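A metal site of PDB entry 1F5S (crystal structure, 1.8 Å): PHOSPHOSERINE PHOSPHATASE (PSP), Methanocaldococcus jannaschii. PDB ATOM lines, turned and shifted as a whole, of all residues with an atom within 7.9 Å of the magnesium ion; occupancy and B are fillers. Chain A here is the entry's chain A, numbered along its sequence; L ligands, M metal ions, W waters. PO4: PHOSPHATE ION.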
ATOM      1  N   PHE A  10     -14.181  30.027 -24.609  1.00  0.00           N
ATOM      2  CA  PHE A  10     -15.187  29.005 -24.771  1.00  0.00           C
ATOM      3  C   PHE A  10     -14.652  27.809 -25.523  1.00  0.00           C
ATOM      4  O   PHE A  10     -13.874  27.946 -26.464  1.00  0.00           O
ATOM      5  CB  PHE A  10     -16.354  29.464 -25.660  1.00  0.00           C
ATOM      6  CG  PHE A  10     -17.117  30.617 -25.098  1.00  0.00           C
ATOM      7  CD1 PHE A  10     -18.349  30.412 -24.455  1.00  0.00           C
ATOM      8  CD2 PHE A  10     -16.623  31.888 -25.233  1.00  0.00           C
ATOM      9  CE1 PHE A  10     -19.086  31.476 -23.969  1.00  0.00           C
ATOM     10  CE2 PHE A  10     -17.353  32.985 -24.746  1.00  0.00           C
ATOM     11  CZ  PHE A  10     -18.600  32.774 -24.098  1.00  0.00           C
ATOM     12  N   ASP A  11     -15.185  26.671 -25.137  1.00  0.00           N
ATOM     13  CA  ASP A  11     -14.912  25.389 -25.754  1.00  0.00           C
ATOM     14  C   ASP A  11     -15.839  25.469 -26.993  1.00  0.00           C
ATOM     15  O   ASP A  11     -16.872  26.154 -26.948  1.00  0.00           O
ATOM     16  CB  ASP A  11     -15.357  24.329 -24.737  1.00  0.00           C
ATOM     17  CG  ASP A  11     -15.484  22.984 -25.338  1.00  0.00           C
ATOM     18  OD1 ASP A  11     -16.502  22.310 -25.061  1.00  0.00           O
ATOM     19  OD2 ASP A  11     -14.591  22.617 -26.083  1.00  0.00           O
ATOM     20  N   PHE A  12     -15.489  24.827 -28.119  1.00  0.00           N
ATOM     21  CA  PHE A  12     -16.362  24.888 -29.305  1.00  0.00           C
ATOM     22  C   PHE A  12     -17.495  23.844 -29.358  1.00  0.00           C
ATOM     23  O   PHE A  12     -18.676  24.198 -29.204  1.00  0.00           O
ATOM     24  CB  PHE A  12     -15.490  24.771 -30.586  1.00  0.00           C
ATOM     25  CG  PHE A  12     -16.265  24.881 -31.880  1.00  0.00           C
ATOM     26  CD1 PHE A  12     -16.772  26.102 -32.325  1.00  0.00           C
ATOM     27  CD2 PHE A  12     -16.450  23.761 -32.676  1.00  0.00           C
ATOM     28  CE1 PHE A  12     -17.443  26.195 -33.594  1.00  0.00           C
ATOM     29  CE2 PHE A  12     -17.118  23.843 -33.926  1.00  0.00           C
ATOM     30  CZ  PHE A  12     -17.605  25.057 -34.378  1.00  0.00           C
ATOM     31  N   ASP A  13     -17.127  22.562 -29.521  1.00  0.00           N
ATOM     32  CA  ASP A  13     -18.107  21.489 -29.659  1.00  0.00           C
ATOM     33  C   ASP A  13     -19.031  21.326 -28.453  1.00  0.00           C
ATOM     34  O   ASP A  13     -18.581  21.189 -27.329  1.00  0.00           O
ATOM     35  CB  ASP A  13     -17.390  20.160 -29.987  1.00  0.00           C
ATOM     36  CG  ASP A  13     -16.686  20.201 -31.331  1.00  0.00           C
ATOM     37  OD1 ASP A  13     -15.409  20.068 -31.383  1.00  0.00           O
ATOM     38  OD2 ASP A  13     -17.380  20.374 -32.361  1.00  0.00           O
ATOM     39  N   SER A  14     -20.333  21.306 -28.720  1.00  0.00           N
ATOM     40  CA  SER A  14     -21.363  21.187 -27.716  1.00  0.00           C
ATOM     41  C   SER A  14     -21.460  22.365 -26.776  1.00  0.00           C
ATOM     42  O   SER A  14     -22.278  22.353 -25.872  1.00  0.00           O
ATOM     43  CB  SER A  14     -21.224  19.897 -26.900  1.00  0.00           C
ATOM     44  OG  SER A  14     -21.490  18.791 -27.736  1.00  0.00           O
ATOM     45  N   THR A  15     -20.632  23.401 -26.979  1.00  0.00           N
ATOM     46  CA  THR A  15     -20.723  24.595 -26.130  1.00  0.00           C
ATOM     47  C   THR A  15     -21.097  25.793 -27.003  1.00  0.00           C
ATOM     48  O   THR A  15     -22.210  26.339 -26.863  1.00  0.00           O
ATOM     49  CB  THR A  15     -19.375  24.853 -25.389  1.00  0.00           C
ATOM     50  OG1 THR A  15     -19.154  23.774 -24.489  1.00  0.00           O
ATOM     51  CG2 THR A  15     -19.404  26.162 -24.593  1.00  0.00           C
ATOM     52  N   LEU A  16     -20.218  26.227 -27.903  1.00  0.00           N
ATOM     53  CA  LEU A  16     -20.602  27.325 -28.789  1.00  0.00           C
ATOM     54  C   LEU A  16     -21.591  26.888 -29.889  1.00  0.00           C
ATOM     55  O   LEU A  16     -22.335  27.705 -30.460  1.00  0.00           O
ATOM     56  CB  LEU A  16     -19.392  27.919 -29.496  1.00  0.00           C
ATOM     57  CG  LEU A  16     -18.587  29.049 -28.898  1.00  0.00           C
ATOM     58  CD1 LEU A  16     -17.630  29.629 -29.957  1.00  0.00           C
ATOM     59  CD2 LEU A  16     -19.594  30.149 -28.414  1.00  0.00           C
ATOM     60  N   VAL A  17     -21.527  25.613 -30.237  1.00  0.00           N
ATOM     61  CA  VAL A  17     -22.410  25.051 -31.249  1.00  0.00           C
ATOM     62  C   VAL A  17     -23.027  23.833 -30.608  1.00  0.00           C
ATOM     63  O   VAL A  17     -22.502  23.281 -29.653  1.00  0.00           O
ATOM     64  CB  VAL A  17     -21.637  24.646 -32.545  1.00  0.00           C
ATOM     65  CG1 VAL A  17     -21.048  25.874 -33.202  1.00  0.00           C
ATOM     66  CG2 VAL A  17     -20.471  23.679 -32.185  1.00  0.00           C
ATOM     67  N   ASN A  19     -23.536  20.815 -31.895  1.00  0.00           N
ATOM     68  CA  ASN A  19     -22.961  19.555 -32.384  1.00  0.00           C
ATOM     69  C   ASN A  19     -21.554  19.212 -31.922  1.00  0.00           C
ATOM     70  O   ASN A  19     -20.911  20.011 -31.306  1.00  0.00           O
ATOM     71  CB  ASN A  19     -22.910  19.601 -33.928  1.00  0.00           C
ATOM     72  CG  ASN A  19     -24.048  20.394 -34.545  1.00  0.00           C
ATOM     73  OD1 ASN A  19     -24.183  21.637 -34.382  1.00  0.00           O
ATOM     74  ND2 ASN A  19     -24.902  19.671 -35.285  1.00  0.00           N
ATOM     75  N   GLU A  20     -21.130  17.993 -32.277  1.00  0.00           N
ATOM     76  CA  GLU A  20     -19.755  17.517 -32.065  1.00  0.00           C
ATOM     77  C   GLU A  20     -19.257  17.394 -33.479  1.00  0.00           C
ATOM     78  O   GLU A  20     -19.704  16.533 -34.211  1.00  0.00           O
ATOM     79  CB  GLU A  20     -19.718  16.137 -31.460  1.00  0.00           C
ATOM     80  CG  GLU A  20     -19.780  16.155 -30.008  1.00  0.00           C
ATOM     81  CD  GLU A  20     -18.538  16.729 -29.368  1.00  0.00           C
ATOM     82  OE1 GLU A  20     -17.424  16.756 -29.996  1.00  0.00           O
ATOM     83  OE2 GLU A  20     -18.694  17.133 -28.198  1.00  0.00           O
ATOM     84  N   THR A  39     -15.804   9.552 -28.720  1.00  0.00           N
ATOM     85  CA  THR A  39     -15.967  10.962 -28.335  1.00  0.00           C
ATOM     86  C   THR A  39     -16.520  11.050 -26.916  1.00  0.00           C
ATOM     87  O   THR A  39     -15.997  11.766 -26.046  1.00  0.00           O
ATOM     88  CB  THR A  39     -16.908  11.706 -29.348  1.00  0.00           C
ATOM     89  OG1 THR A  39     -16.293  11.682 -30.663  1.00  0.00           O
ATOM     90  CG2 THR A  39     -17.107  13.161 -28.915  1.00  0.00           C
ATOM     91  N   MET A  43     -14.622  12.766 -23.739  1.00  0.00           N
ATOM     92  CA  MET A  43     -15.160  13.909 -23.027  1.00  0.00           C
ATOM     93  C   MET A  43     -15.430  13.614 -21.564  1.00  0.00           C
ATOM     94  O   MET A  43     -15.424  14.514 -20.730  1.00  0.00           O
ATOM     95  CB  MET A  43     -16.408  14.417 -23.749  1.00  0.00           C
ATOM     96  CG  MET A  43     -16.091  15.011 -25.088  1.00  0.00           C
ATOM     97  SD  MET A  43     -14.798  16.510 -25.002  1.00  0.00           S
ATOM     98  CE  MET A  43     -13.201  15.421 -25.376  1.00  0.00           C
ATOM     99  N   VAL A  98     -11.385  28.002 -27.991  1.00  0.00           N
ATOM    100  CA  VAL A  98     -10.210  27.119 -27.939  1.00  0.00           C
ATOM    101  C   VAL A  98     -10.810  25.741 -28.077  1.00  0.00           C
ATOM    102  O   VAL A  98     -11.592  25.344 -27.235  1.00  0.00           O
ATOM    103  CB  VAL A  98      -9.486  27.229 -26.587  1.00  0.00           C
ATOM    104  CG1 VAL A  98      -8.214  26.355 -26.635  1.00  0.00           C
ATOM    105  CG2 VAL A  98      -9.169  28.729 -26.283  1.00  0.00           C
ATOM    106  N   SER A  99     -10.380  24.998 -29.083  1.00  0.00           N
ATOM    107  CA  SER A  99     -11.038  23.713 -29.372  1.00  0.00           C
ATOM    108  C   SER A  99     -10.123  22.582 -29.817  1.00  0.00           C
ATOM    109  O   SER A  99      -9.201  22.809 -30.619  1.00  0.00           O
ATOM    110  CB  SER A  99     -12.064  23.957 -30.509  1.00  0.00           C
ATOM    111  OG  SER A  99     -12.668  22.757 -31.082  1.00  0.00           O
ATOM    112  N   GLY A 100     -10.424  21.380 -29.329  1.00  0.00           N
ATOM    113  CA  GLY A 100      -9.705  20.193 -29.773  1.00  0.00           C
ATOM    114  C   GLY A 100     -10.284  19.742 -31.096  1.00  0.00           C
ATOM    115  O   GLY A 100      -9.928  18.671 -31.652  1.00  0.00           O
ATOM    116  N   LYS A 144      -5.189  23.392 -23.614  1.00  0.00           N
ATOM    117  CA  LYS A 144      -6.072  24.548 -23.458  1.00  0.00           C
ATOM    118  C   LYS A 144      -5.605  25.540 -22.382  1.00  0.00           C
ATOM    119  O   LYS A 144      -5.715  26.752 -22.538  1.00  0.00           O
ATOM    120  CB  LYS A 144      -7.508  24.089 -23.209  1.00  0.00           C
ATOM    121  CG  LYS A 144      -8.085  23.412 -24.476  1.00  0.00           C
ATOM    122  CD  LYS A 144      -9.639  23.369 -24.442  1.00  0.00           C
ATOM    123  CE  LYS A 144     -10.231  22.525 -25.604  1.00  0.00           C
ATOM    124  NZ  LYS A 144     -11.765  22.677 -25.686  1.00  0.00           N
ATOM    125  N   VAL A 165     -15.341  28.667 -20.108  1.00  0.00           N
ATOM    126  CA  VAL A 165     -16.676  28.040 -20.235  1.00  0.00           C
ATOM    127  C   VAL A 165     -16.440  26.748 -21.019  1.00  0.00           C
ATOM    128  O   VAL A 165     -16.116  26.787 -22.190  1.00  0.00           O
ATOM    129  CB  VAL A 165     -17.639  28.984 -21.025  1.00  0.00           C
ATOM    130  CG1 VAL A 165     -19.034  28.347 -21.064  1.00  0.00           C
ATOM    131  CG2 VAL A 165     -17.710  30.399 -20.348  1.00  0.00           C
ATOM    132  N   GLY A 166     -16.613  25.590 -20.381  1.00  0.00           N
ATOM    133  CA  GLY A 166     -16.322  24.344 -21.090  1.00  0.00           C
ATOM    134  C   GLY A 166     -17.326  23.240 -20.808  1.00  0.00           C
ATOM    135  O   GLY A 166     -18.240  23.425 -19.998  1.00  0.00           O
ATOM    136  N   ASP A 167     -17.158  22.092 -21.455  1.00  0.00           N
ATOM    137  CA  ASP A 167     -18.120  21.033 -21.212  1.00  0.00           C
ATOM    138  C   ASP A 167     -17.517  19.655 -21.261  1.00  0.00           C
ATOM    139  O   ASP A 167     -18.242  18.713 -21.063  1.00  0.00           O
ATOM    140  CB  ASP A 167     -19.306  21.092 -22.173  1.00  0.00           C
ATOM    141  CG  ASP A 167     -18.917  20.838 -23.630  1.00  0.00           C
ATOM    142  OD1 ASP A 167     -19.593  21.336 -24.559  1.00  0.00           O
ATOM    143  OD2 ASP A 167     -17.946  20.149 -23.901  1.00  0.00           O
ATOM    144  N   GLY A 168     -16.215  19.552 -21.505  1.00  0.00           N
ATOM    145  CA  GLY A 168     -15.584  18.232 -21.603  1.00  0.00           C
ATOM    146  C   GLY A 168     -14.301  18.087 -20.828  1.00  0.00           C
ATOM    147  O   GLY A 168     -13.732  19.058 -20.330  1.00  0.00           O
ATOM    148  N   ALA A 169     -13.789  16.855 -20.746  1.00  0.00           N
ATOM    149  CA  ALA A 169     -12.555  16.666 -19.978  1.00  0.00           C
ATOM    150  C   ALA A 169     -11.341  17.387 -20.543  1.00  0.00           C
ATOM    151  O   ALA A 169     -10.430  17.655 -19.795  1.00  0.00           O
ATOM    152  CB  ALA A 169     -12.238  15.175 -19.809  1.00  0.00           C
ATOM    153  N   ASN A 170     -11.304  17.707 -21.848  1.00  0.00           N
ATOM    154  CA  ASN A 170     -10.150  18.436 -22.362  1.00  0.00           C
ATOM    155  C   ASN A 170     -10.220  19.931 -22.053  1.00  0.00           C
ATOM    156  O   ASN A 170      -9.368  20.706 -22.532  1.00  0.00           O
ATOM    157  CB  ASN A 170      -9.971  18.229 -23.887  1.00  0.00           C
ATOM    158  CG  ASN A 170     -11.147  18.724 -24.712  1.00  0.00           C
ATOM    159  OD1 ASN A 170     -12.295  18.627 -24.282  1.00  0.00           O
ATOM    160  ND2 ASN A 170     -10.872  19.204 -25.948  1.00  0.00           N
ATOM    161  N   ASP A 171     -11.218  20.327 -21.252  1.00  0.00           N
ATOM    162  CA  ASP A 171     -11.345  21.709 -20.800  1.00  0.00           C
ATOM    163  C   ASP A 171     -10.787  21.767 -19.383  1.00  0.00           C
ATOM    164  O   ASP A 171     -10.709  22.848 -18.795  1.00  0.00           O
ATOM    165  CB  ASP A 171     -12.784  22.175 -20.794  1.00  0.00           C
ATOM    166  CG  ASP A 171     -13.353  22.204 -22.175  1.00  0.00           C
ATOM    167  OD1 ASP A 171     -12.646  22.685 -23.055  1.00  0.00           O
ATOM    168  OD2 ASP A 171     -14.478  21.738 -22.406  1.00  0.00           O
ATOM    169  N   PHE A 184     -20.772  24.279 -18.740  1.00  0.00           N
ATOM    170  CA  PHE A 184     -21.982  24.469 -19.512  1.00  0.00           C
ATOM    171  C   PHE A 184     -22.506  23.115 -20.036  1.00  0.00           C
ATOM    172  O   PHE A 184     -21.873  22.518 -20.933  1.00  0.00           O
ATOM    173  CB  PHE A 184     -21.671  25.374 -20.696  1.00  0.00           C
ATOM    174  CG  PHE A 184     -22.874  25.700 -21.552  1.00  0.00           C
ATOM    175  CD1 PHE A 184     -23.863  26.568 -21.096  1.00  0.00           C
ATOM    176  CD2 PHE A 184     -23.001  25.157 -22.807  1.00  0.00           C
ATOM    177  CE1 PHE A 184     -24.981  26.889 -21.907  1.00  0.00           C
ATOM    178  CE2 PHE A 184     -24.099  25.470 -23.626  1.00  0.00           C
ATOM    179  CZ  PHE A 184     -25.079  26.333 -23.168  1.00  0.00           C
ATOM    180  N   LYS A 187     -19.975  17.344 -18.852  1.00  0.00           N
ATOM    181  CA  LYS A 187     -19.784  15.971 -18.354  1.00  0.00           C
ATOM    182  C   LYS A 187     -19.431  16.046 -16.870  1.00  0.00           C
ATOM    183  O   LYS A 187     -18.872  17.038 -16.379  1.00  0.00           O
ATOM    184  CB  LYS A 187     -18.655  15.271 -19.107  1.00  0.00           C
ATOM    185  CG  LYS A 187     -18.967  14.991 -20.570  1.00  0.00           C
ATOM    186  CD  LYS A 187     -20.249  14.176 -20.700  1.00  0.00           C
ATOM    187  CE  LYS A 187     -20.495  13.865 -22.197  1.00  0.00           C
ATOM    188  NZ  LYS A 187     -21.788  13.164 -22.370  1.00  0.00           N
ATOM    189  N   LEU A 190     -16.004  17.315 -15.460  1.00  0.00           N
ATOM    190  CA  LEU A 190     -15.738  18.756 -15.464  1.00  0.00           C
ATOM    191  C   LEU A 190     -16.621  19.442 -14.446  1.00  0.00           C
ATOM    192  O   LEU A 190     -16.201  20.401 -13.810  1.00  0.00           O
ATOM    193  CB  LEU A 190     -15.964  19.368 -16.847  1.00  0.00           C
ATOM    194  CG  LEU A 190     -15.481  20.819 -16.981  1.00  0.00           C
ATOM    195  CD1 LEU A 190     -13.953  20.885 -16.960  1.00  0.00           C
ATOM    196  CD2 LEU A 190     -16.035  21.422 -18.288  1.00  0.00           C
HETATM  197  P   PO4 L   1     -13.896  20.876 -28.303  1.00  0.00           P
HETATM  198  O1  PO4 L   1     -15.008  20.515 -27.195  1.00  0.00           O
HETATM  199  O2  PO4 L   1     -14.285  22.225 -29.064  1.00  0.00           O
HETATM  200  O3  PO4 L   1     -12.400  20.880 -27.612  1.00  0.00           O
HETATM  201  O4  PO4 L   1     -13.904  19.638 -29.358  1.00  0.00           O
HETATM  202 MG    MG M   1     -16.866  20.323 -25.911  1.00  0.00          MG
HETATM  203  O   HOH W   1     -14.581  20.184 -24.633  1.00  0.00           O
HETATM  204  O   HOH W   2     -17.613  18.207 -26.248  1.00  0.00           O
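The side-chain carboxylate (OD1) of Asp 11 sits close to the side-chain hydroxyl (OG1) of Thr 15 (3.1 Å). The side-chain carboxylate (OD2) of Asp 11 is in salt-bridge range of the side-chain amino group (NZ) of Lys 144 (2.9 Å). The backbone carbonyl oxygen (O) of Asp 11 sits at hydrogen-bond distance from the backbone NH (N) of Leu 16, at 3.5 Å. The backbone NH (N) of Asp 11 is in hydrogen-bond range of the backbone carbonyl oxygen (O) of Val 165. The side-chain hydroxyl (OG1) of Thr 15 sits at hydrogen-bond distance from the side-chain carboxylate (OD1) of Asp 167, 2.5 Å away. The side-chain carboxylate of Asp 171 lies within hydrogen-bond range of the backbone NH of Asp 167. The backbone NH (N) of Lys 187 sits at hydrogen-bond distance from the backbone carbonyl oxygen (O) of Asp 167.
Within 4 Å of the magnesium ion: Asp 11, Asp 13 and Asp 167. The nearest printed residue that does not touch the magnesium ion is Glu 20 (4.3 Å).
OD1 of Asp 11 binds the magnesium ion, 2.2 Å away. O1 of the ligand is bound to the magnesium ion, 2.3 Å away. Water W2 is bound to the magnesium ion (2.3 Å). OD2 of Asp 167 is bound to the magnesium ion (2.3 Å). O of Asp 13 is bound to the magnesium ion (2.4 Å). The magnesium ion has five donor atoms within binding distance. Slightly farther from the magnesium ion lies water W1 (2.6 Å).
Water W2 lies within hydrogen-bond range of the side-chain carboxylate (OE2) of Glu 20 (2.5 Å) and the side-chain sulfur (SD) of Met 43 (3.5 Å).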
